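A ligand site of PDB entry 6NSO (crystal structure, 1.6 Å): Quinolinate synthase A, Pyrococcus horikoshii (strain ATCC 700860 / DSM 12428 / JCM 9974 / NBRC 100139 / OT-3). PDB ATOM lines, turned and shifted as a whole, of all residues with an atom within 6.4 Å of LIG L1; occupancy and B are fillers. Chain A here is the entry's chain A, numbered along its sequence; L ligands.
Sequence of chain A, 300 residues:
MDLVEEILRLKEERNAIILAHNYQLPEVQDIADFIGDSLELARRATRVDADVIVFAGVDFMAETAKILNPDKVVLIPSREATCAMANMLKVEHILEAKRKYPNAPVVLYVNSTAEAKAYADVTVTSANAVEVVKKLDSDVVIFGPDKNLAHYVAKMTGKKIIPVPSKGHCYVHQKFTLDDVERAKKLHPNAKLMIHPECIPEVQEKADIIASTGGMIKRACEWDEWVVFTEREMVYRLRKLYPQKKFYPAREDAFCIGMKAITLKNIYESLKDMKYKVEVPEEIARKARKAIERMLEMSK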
ATOM      1  N   HIS A  21     -18.124 -16.734 -17.978  1.00  0.00           N
ATOM      2  CA  HIS A  21     -18.498 -15.349 -18.242  1.00  0.00           C
ATOM      3  C   HIS A  21     -17.332 -14.606 -18.890  1.00  0.00           C
ATOM      4  O   HIS A  21     -16.159 -15.009 -18.789  1.00  0.00           O
ATOM      5  CB  HIS A  21     -18.906 -14.630 -16.945  1.00  0.00           C
ATOM      6  CG  HIS A  21     -19.458 -13.253 -17.175  1.00  0.00           C
ATOM      7  ND1 HIS A  21     -18.670 -12.131 -17.106  1.00  0.00           N
ATOM      8  CD2 HIS A  21     -20.701 -12.824 -17.509  1.00  0.00           C
ATOM      9  CE1 HIS A  21     -19.396 -11.057 -17.369  1.00  0.00           C
ATOM     10  NE2 HIS A  21     -20.632 -11.462 -17.620  1.00  0.00           N
ATOM     11  N   TYR A  23     -15.875 -12.006 -18.026  1.00  0.00           N
ATOM     12  CA  TYR A  23     -14.915 -11.435 -17.084  1.00  0.00           C
ATOM     13  C   TYR A  23     -13.974 -12.488 -16.507  1.00  0.00           C
ATOM     14  O   TYR A  23     -13.187 -12.172 -15.610  1.00  0.00           O
ATOM     15  CB  TYR A  23     -15.621 -10.733 -15.922  1.00  0.00           C
ATOM     16  CG  TYR A  23     -16.515  -9.547 -16.289  1.00  0.00           C
ATOM     17  CD1 TYR A  23     -16.409  -8.902 -17.514  1.00  0.00           C
ATOM     18  CD2 TYR A  23     -17.480  -9.085 -15.377  1.00  0.00           C
ATOM     19  CE1 TYR A  23     -17.226  -7.817 -17.822  1.00  0.00           C
ATOM     20  CE2 TYR A  23     -18.305  -8.007 -15.671  1.00  0.00           C
ATOM     21  CZ  TYR A  23     -18.182  -7.395 -16.903  1.00  0.00           C
ATOM     22  OH  TYR A  23     -19.000  -6.329 -17.206  1.00  0.00           O
ATOM     23  N   VAL A  58     -19.976 -16.160 -11.316  1.00  0.00           N
ATOM     24  CA  VAL A  58     -20.327 -15.932  -9.914  1.00  0.00           C
ATOM     25  C   VAL A  58     -21.636 -16.639  -9.599  1.00  0.00           C
ATOM     26  O   VAL A  58     -22.334 -17.123 -10.499  1.00  0.00           O
ATOM     27  CB  VAL A  58     -20.406 -14.436  -9.536  1.00  0.00           C
ATOM     28  CG1 VAL A  58     -19.033 -13.809  -9.625  1.00  0.00           C
ATOM     29  CG2 VAL A  58     -21.419 -13.714 -10.418  1.00  0.00           C
ATOM     30  N   PHE A  60     -24.825 -16.070  -8.614  1.00  0.00           N
ATOM     31  CA  PHE A  60     -26.174 -15.896  -9.156  1.00  0.00           C
ATOM     32  C   PHE A  60     -26.273 -16.457 -10.571  1.00  0.00           C
ATOM     33  O   PHE A  60     -27.356 -16.870 -11.005  1.00  0.00           O
ATOM     34  CB  PHE A  60     -26.606 -14.413  -9.113  1.00  0.00           C
ATOM     35  CG  PHE A  60     -25.925 -13.518 -10.146  1.00  0.00           C
ATOM     36  CD1 PHE A  60     -26.353 -13.507 -11.482  1.00  0.00           C
ATOM     37  CD2 PHE A  60     -24.923 -12.645  -9.772  1.00  0.00           C
ATOM     38  CE1 PHE A  60     -25.735 -12.687 -12.408  1.00  0.00           C
ATOM     39  CE2 PHE A  60     -24.307 -11.808 -10.712  1.00  0.00           C
ATOM     40  CZ  PHE A  60     -24.712 -11.832 -12.024  1.00  0.00           C
ATOM     41  N   MET A  61     -25.131 -16.513 -11.285  1.00  0.00           N
ATOM     42  CA  MET A  61     -25.100 -17.031 -12.636  1.00  0.00           C
ATOM     43  C   MET A  61     -25.197 -18.546 -12.650  1.00  0.00           C
ATOM     44  O   MET A  61     -25.960 -19.115 -13.439  1.00  0.00           O
ATOM     45  CB  MET A  61     -23.809 -16.578 -13.318  1.00  0.00           C
ATOM     46  CG  MET A  61     -23.696 -15.071 -13.464  1.00  0.00           C
ATOM     47  SD  MET A  61     -22.199 -14.666 -14.406  1.00  0.00           S
ATOM     48  CE  MET A  61     -22.421 -12.900 -14.576  1.00  0.00           C
ATOM     49  N   THR A  82     -18.781 -14.471  -5.841  1.00  0.00           N
ATOM     50  CA  THR A  82     -20.058 -13.849  -5.516  1.00  0.00           C
ATOM     51  C   THR A  82     -20.096 -12.421  -6.040  1.00  0.00           C
ATOM     52  O   THR A  82     -19.071 -11.770  -6.273  1.00  0.00           O
ATOM     53  CB  THR A  82     -20.299 -13.872  -3.995  1.00  0.00           C
ATOM     54  OG1 THR A  82     -19.254 -13.135  -3.335  1.00  0.00           O
ATOM     55  CG2 THR A  82     -20.278 -15.305  -3.455  1.00  0.00           C
ATOM     56  N   CYS A  83     -21.331 -11.943  -6.218  1.00  0.00           N
ATOM     57  CA  CYS A  83     -21.608 -10.629  -6.763  1.00  0.00           C
ATOM     58  C   CYS A  83     -22.060  -9.705  -5.641  1.00  0.00           C
ATOM     59  O   CYS A  83     -23.152  -9.894  -5.081  1.00  0.00           O
ATOM     60  CB  CYS A  83     -22.676 -10.698  -7.853  1.00  0.00           C
ATOM     61  SG  CYS A  83     -23.190  -9.075  -8.458  1.00  0.00           S
ATOM     62  N   ALA A  84     -21.260  -8.674  -5.394  1.00  0.00           N
ATOM     63  CA  ALA A  84     -21.543  -7.731  -4.307  1.00  0.00           C
ATOM     64  C   ALA A  84     -22.881  -7.041  -4.511  1.00  0.00           C
ATOM     65  O   ALA A  84     -23.640  -6.832  -3.556  1.00  0.00           O
ATOM     66  CB  ALA A  84     -20.430  -6.687  -4.233  1.00  0.00           C
ATOM     67  N   MET A  85     -23.194  -6.694  -5.766  1.00  0.00           N
ATOM     68  CA  MET A  85     -24.405  -5.938  -6.069  1.00  0.00           C
ATOM     69  C   MET A  85     -25.645  -6.807  -5.944  1.00  0.00           C
ATOM     70  O   MET A  85     -26.681  -6.363  -5.443  1.00  0.00           O
ATOM     71  CB  MET A  85     -24.293  -5.351  -7.483  1.00  0.00           C
ATOM     72  CG  MET A  85     -25.564  -4.654  -7.991  1.00  0.00           C
ATOM     73  SD  MET A  85     -26.479  -5.565  -9.263  1.00  0.00           S
ATOM     74  CE  MET A  85     -25.350  -5.341 -10.643  1.00  0.00           C
ATOM     75  N   ALA A  86     -25.550  -8.070  -6.381  1.00  0.00           N
ATOM     76  CA  ALA A  86     -26.679  -9.001  -6.288  1.00  0.00           C
ATOM     77  C   ALA A  86     -27.096  -9.225  -4.847  1.00  0.00           C
ATOM     78  O   ALA A  86     -28.293  -9.363  -4.548  1.00  0.00           O
ATOM     79  CB  ALA A  86     -26.311 -10.336  -6.953  1.00  0.00           C
ATOM     80  N   TYR A 109     -33.090  -7.532 -12.287  1.00  0.00           N
ATOM     81  CA  TYR A 109     -31.828  -7.850 -12.925  1.00  0.00           C
ATOM     82  C   TYR A 109     -31.418  -9.267 -12.534  1.00  0.00           C
ATOM     83  O   TYR A 109     -31.585  -9.690 -11.379  1.00  0.00           O
ATOM     84  CB  TYR A 109     -30.790  -6.836 -12.435  1.00  0.00           C
ATOM     85  CG  TYR A 109     -29.583  -6.569 -13.295  1.00  0.00           C
ATOM     86  CD1 TYR A 109     -29.519  -6.970 -14.629  1.00  0.00           C
ATOM     87  CD2 TYR A 109     -28.510  -5.876 -12.768  1.00  0.00           C
ATOM     88  CE1 TYR A 109     -28.394  -6.709 -15.394  1.00  0.00           C
ATOM     89  CE2 TYR A 109     -27.401  -5.618 -13.507  1.00  0.00           C
ATOM     90  CZ  TYR A 109     -27.332  -6.024 -14.820  1.00  0.00           C
ATOM     91  OH  TYR A 109     -26.204  -5.739 -15.528  1.00  0.00           O
ATOM     92  N   ASN A 111     -28.659 -10.203 -11.904  1.00  0.00           N
ATOM     93  CA  ASN A 111     -27.778 -10.073 -10.752  1.00  0.00           C
ATOM     94  C   ASN A 111     -28.631  -9.989  -9.480  1.00  0.00           C
ATOM     95  O   ASN A 111     -28.783  -8.928  -8.864  1.00  0.00           O
ATOM     96  CB  ASN A 111     -26.864  -8.851 -10.895  1.00  0.00           C
ATOM     97  CG  ASN A 111     -26.038  -8.872 -12.165  1.00  0.00           C
ATOM     98  OD1 ASN A 111     -26.547  -9.188 -13.245  1.00  0.00           O
ATOM     99  ND2 ASN A 111     -24.754  -8.541 -12.045  1.00  0.00           N
ATOM    100  N   ASP A 146     -29.604  -2.687  -9.523  1.00  0.00           N
ATOM    101  CA  ASP A 146     -28.613  -1.717  -9.973  1.00  0.00           C
ATOM    102  C   ASP A 146     -29.263  -0.384 -10.306  1.00  0.00           C
ATOM    103  O   ASP A 146     -29.968  -0.264 -11.307  1.00  0.00           O
ATOM    104  CB  ASP A 146     -27.852  -2.255 -11.176  1.00  0.00           C
ATOM    105  CG  ASP A 146     -26.612  -1.457 -11.464  1.00  0.00           C
ATOM    106  OD1 ASP A 146     -26.744  -0.305 -11.900  1.00  0.00           O
ATOM    107  OD2 ASP A 146     -25.497  -1.957 -11.220  1.00  0.00           O
ATOM    108  N   HIS A 169     -25.540  -0.954  -6.509  1.00  0.00           N
ATOM    109  CA  HIS A 169     -24.571  -0.611  -7.542  1.00  0.00           C
ATOM    110  C   HIS A 169     -23.448  -1.635  -7.544  1.00  0.00           C
ATOM    111  O   HIS A 169     -23.265  -2.394  -6.592  1.00  0.00           O
ATOM    112  CB  HIS A 169     -23.989   0.775  -7.338  1.00  0.00           C
ATOM    113  CG  HIS A 169     -23.103   0.873  -6.149  1.00  0.00           C
ATOM    114  ND1 HIS A 169     -23.596   1.092  -4.879  1.00  0.00           N
ATOM    115  CD2 HIS A 169     -21.768   0.753  -6.017  1.00  0.00           C
ATOM    116  CE1 HIS A 169     -22.592   1.108  -4.015  1.00  0.00           C
ATOM    117  NE2 HIS A 169     -21.470   0.919  -4.681  1.00  0.00           N
ATOM    118  N   CYS A 170     -22.668  -1.608  -8.624  1.00  0.00           N
ATOM    119  CA  CYS A 170     -21.507  -2.458  -8.793  1.00  0.00           C
ATOM    120  C   CYS A 170     -20.246  -1.629  -8.533  1.00  0.00           C
ATOM    121  O   CYS A 170     -20.011  -0.646  -9.248  1.00  0.00           O
ATOM    122  CB  CYS A 170     -21.495  -3.062 -10.203  1.00  0.00           C
ATOM    123  SG  CYS A 170     -19.881  -3.686 -10.629  1.00  0.00           S
ATOM    124  N   TYR A 171     -19.481  -1.999  -7.498  1.00  0.00           N
ATOM    125  CA  TYR A 171     -18.270  -1.251  -7.154  1.00  0.00           C
ATOM    126  C   TYR A 171     -17.258  -1.225  -8.300  1.00  0.00           C
ATOM    127  O   TYR A 171     -16.443  -0.302  -8.369  1.00  0.00           O
ATOM    128  CB  TYR A 171     -17.587  -1.826  -5.912  1.00  0.00           C
ATOM    129  CG  TYR A 171     -16.929  -3.173  -6.095  1.00  0.00           C
ATOM    130  CD1 TYR A 171     -17.649  -4.361  -5.922  1.00  0.00           C
ATOM    131  CD2 TYR A 171     -15.585  -3.275  -6.392  1.00  0.00           C
ATOM    132  CE1 TYR A 171     -17.048  -5.606  -6.073  1.00  0.00           C
ATOM    133  CE2 TYR A 171     -14.970  -4.507  -6.529  1.00  0.00           C
ATOM    134  CZ  TYR A 171     -15.691  -5.658  -6.375  1.00  0.00           C
ATOM    135  OH  TYR A 171     -15.058  -6.884  -6.528  1.00  0.00           O
ATOM    136  N   VAL A 172     -17.257  -2.248  -9.153  1.00  0.00           N
ATOM    137  CA  VAL A 172     -16.341  -2.280 -10.294  1.00  0.00           C
ATOM    138  C   VAL A 172     -16.668  -1.165 -11.275  1.00  0.00           C
ATOM    139  O   VAL A 172     -15.805  -0.358 -11.644  1.00  0.00           O
ATOM    140  CB  VAL A 172     -16.372  -3.653 -10.981  1.00  0.00           C
ATOM    141  CG1 VAL A 172     -15.392  -3.695 -12.156  1.00  0.00           C
ATOM    142  CG2 VAL A 172     -16.077  -4.759  -9.962  1.00  0.00           C
ATOM    143  N   HIS A 173     -17.930  -1.099 -11.707  1.00  0.00           N
ATOM    144  CA  HIS A 173     -18.329  -0.097 -12.697  1.00  0.00           C
ATOM    145  C   HIS A 173     -18.441   1.306 -12.110  1.00  0.00           C
ATOM    146  O   HIS A 173     -18.281   2.287 -12.838  1.00  0.00           O
ATOM    147  CB  HIS A 173     -19.628  -0.550 -13.354  1.00  0.00           C
ATOM    148  CG  HIS A 173     -19.405  -1.706 -14.270  1.00  0.00           C
ATOM    149  ND1 HIS A 173     -19.603  -3.016 -13.877  1.00  0.00           N
ATOM    150  CD2 HIS A 173     -18.953  -1.762 -15.548  1.00  0.00           C
ATOM    151  CE1 HIS A 173     -19.312  -3.816 -14.884  1.00  0.00           C
ATOM    152  NE2 HIS A 173     -18.895  -3.085 -15.899  1.00  0.00           N
ATOM    153  N   GLU A 198     -23.923  -0.287 -16.149  1.00  0.00           N
ATOM    154  CA  GLU A 198     -23.693  -0.227 -14.708  1.00  0.00           C
ATOM    155  C   GLU A 198     -22.779   0.931 -14.318  1.00  0.00           C
ATOM    156  O   GLU A 198     -22.617   1.190 -13.120  1.00  0.00           O
ATOM    157  CB  GLU A 198     -23.104  -1.545 -14.194  1.00  0.00           C
ATOM    158  CG  GLU A 198     -24.129  -2.669 -14.123  1.00  0.00           C
ATOM    159  CD  GLU A 198     -23.527  -4.047 -13.851  1.00  0.00           C
ATOM    160  OE1 GLU A 198     -22.399  -4.127 -13.321  1.00  0.00           O
ATOM    161  OE2 GLU A 198     -24.197  -5.057 -14.166  1.00  0.00           O
ATOM    162  N   GLU A 231     -15.300  -4.344 -16.763  1.00  0.00           N
ATOM    163  CA  GLU A 231     -14.294  -5.144 -16.073  1.00  0.00           C
ATOM    164  C   GLU A 231     -13.154  -5.495 -17.021  1.00  0.00           C
ATOM    165  O   GLU A 231     -13.374  -5.855 -18.171  1.00  0.00           O
ATOM    166  CB  GLU A 231     -14.929  -6.409 -15.490  1.00  0.00           C
ATOM    167  CG  GLU A 231     -14.320  -6.925 -14.181  1.00  0.00           C
ATOM    168  CD  GLU A 231     -13.167  -7.908 -14.390  1.00  0.00           C
ATOM    169  OE1 GLU A 231     -12.857  -8.244 -15.566  1.00  0.00           O
ATOM    170  OE2 GLU A 231     -12.567  -8.333 -13.386  1.00  0.00           O
ATOM    171  N   CYS A 256     -13.209  -7.446 -10.837  1.00  0.00           N
ATOM    172  CA  CYS A 256     -14.244  -8.104 -10.041  1.00  0.00           C
ATOM    173  C   CYS A 256     -13.624  -9.234  -9.221  1.00  0.00           C
ATOM    174  O   CYS A 256     -13.269 -10.281  -9.762  1.00  0.00           O
ATOM    175  CB  CYS A 256     -15.363  -8.655 -10.918  1.00  0.00           C
ATOM    176  SG  CYS A 256     -16.646  -9.517  -9.971  1.00  0.00           S
ATOM    177  N   ILE A 257     -13.554  -9.045  -7.900  1.00  0.00           N
ATOM    178  CA  ILE A 257     -12.951 -10.046  -7.012  1.00  0.00           C
ATOM    179  C   ILE A 257     -13.729 -11.349  -7.061  1.00  0.00           C
ATOM    180  O   ILE A 257     -13.150 -12.439  -7.086  1.00  0.00           O
ATOM    181  CB  ILE A 257     -12.850  -9.472  -5.590  1.00  0.00           C
ATOM    182  CG1 ILE A 257     -12.044  -8.173  -5.598  1.00  0.00           C
ATOM    183  CG2 ILE A 257     -12.171 -10.468  -4.637  1.00  0.00           C
ATOM    184  CD1 ILE A 257     -12.056  -7.409  -4.290  1.00  0.00           C
ATOM    185  N   GLY A 258     -15.054 -11.275  -7.132  1.00  0.00           N
ATOM    186  CA  GLY A 258     -15.842 -12.502  -7.208  1.00  0.00           C
ATOM    187  C   GLY A 258     -15.565 -13.321  -8.461  1.00  0.00           C
ATOM    188  O   GLY A 258     -15.407 -14.544  -8.395  1.00  0.00           O
ATOM    189  N   MET A 259     -15.503 -12.658  -9.617  1.00  0.00           N
ATOM    190  CA  MET A 259     -15.183 -13.351 -10.857  1.00  0.00           C
ATOM    191  C   MET A 259     -13.836 -14.063 -10.745  1.00  0.00           C
ATOM    192  O   MET A 259     -13.701 -15.222 -11.174  1.00  0.00           O
ATOM    193  CB  MET A 259     -15.157 -12.348 -12.013  1.00  0.00           C
ATOM    194  CG  MET A 259     -16.547 -11.941 -12.496  1.00  0.00           C
ATOM    195  SD  MET A 259     -17.420 -13.329 -13.273  1.00  0.00           S
ATOM    196  CE  MET A 259     -18.944 -12.525 -13.661  1.00  0.00           C
HETATM  197 FE1  LIG L   1     -20.706  -8.043 -12.257  1.00  0.00          FE
HETATM  198 FE2  LIG L   1     -21.317  -8.246  -9.655  1.00  0.00          FE
HETATM  199 FE3  LIG L   1     -20.035  -6.111 -10.538  1.00  0.00          FE
HETATM  200 FE4  LIG L   1     -18.702  -8.433 -10.352  1.00  0.00          FE
HETATM  201  S1  LIG L   1     -19.586  -7.249  -8.672  1.00  0.00           S
HETATM  202  S2  LIG L   1     -18.728  -7.059 -12.059  1.00  0.00           S
HETATM  203  S3  LIG L   1     -20.379  -9.744 -10.934  1.00  0.00           S
HETATM  204  S4  LIG L   1     -22.055  -6.749 -11.094  1.00  0.00           S
HETATM  205  P1  LG2 L   2     -23.231  -8.538 -18.862  1.00  0.00           P
HETATM  206  O1  LG2 L   2     -22.987  -7.122 -19.408  1.00  0.00           O
HETATM  207  O2  LG2 L   2     -24.595  -9.152 -19.011  1.00  0.00           O
HETATM  208  O3  LG2 L   2     -22.012  -9.409 -18.902  1.00  0.00           O
HETATM  209  O4  LG2 L   2     -23.176  -8.094 -17.092  1.00  0.00           O
HETATM  210  C1  LG2 L   2     -21.879  -8.090 -16.664  1.00  0.00           C
HETATM  211  C2  LG2 L   2     -21.898  -7.682 -15.216  1.00  0.00           C
HETATM  212  O5  LG2 L   2     -21.554  -6.613 -14.773  1.00  0.00           O
HETATM  213  C3  LG2 L   2     -22.372  -8.744 -14.256  1.00  0.00           C
HETATM  214  O6  LG2 L   2     -21.264  -9.490 -14.004  1.00  0.00           O
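The side-chain sulfur of Cys 256 binds an iron atom (FE4) of LIG L1 (2.4 Å). An iron atom (FE2) of LIG L1 is bound by the side-chain sulfur (SG) of Cys 83. The side-chain sulfur of Cys 170 is bound to an iron atom (FE3) of LIG L1, at 2.4 Å. The side-chain amide nitrogen of Asn 111 lies close to a sulfur (S4) of LIG L1 (3.4 Å). NE2 of His 21 lies within hydrogen-bond range of O3 of LG2 L2 (2.8 Å).
An iron atom (FE1) of LIG L1 is bound by an oxygen (O6) of LG2 L2 (2.3 Å).
N of Cys 256 is in hydrogen-bond range of OE2 of Glu 231 (2.8 Å). The backbone NH (N) of Met 85 lies close to the side-chain sulfur (SG) of Cys 83, at 3.6 Å. The side-chain sulfur of Cys 170 lies close to the side-chain carboxylate of Glu 198 (3.7 Å). N of Val 172 lies close to SG of Cys 170, at 3.3 Å. ND1 of His 173 sits close to SG of Cys 170 (3.3 Å). The side-chain carboxylate of Glu 198 sits at hydrogen-bond distance from the side-chain hydroxyl of Tyr 109. The side-chain hydroxyl (OH) of Tyr 23 sits close to a ring nitrogen (NE2) of His 173. N of Tyr 23 sits at hydrogen-bond distance from ND1 of His 21, at 2.9 Å.
The side-chain carboxylate of Glu 198 sits close to a sulfur (S4) of LIG L1. Merely in contact with LIG L1: Met 85 (3.6 Å), Tyr 23 (3.8 Å), Ala 84 (3.9 Å) and Tyr 171 (3.99 Å). Of the 24 residues printed, 9 come within 4 Å of LIG L1.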
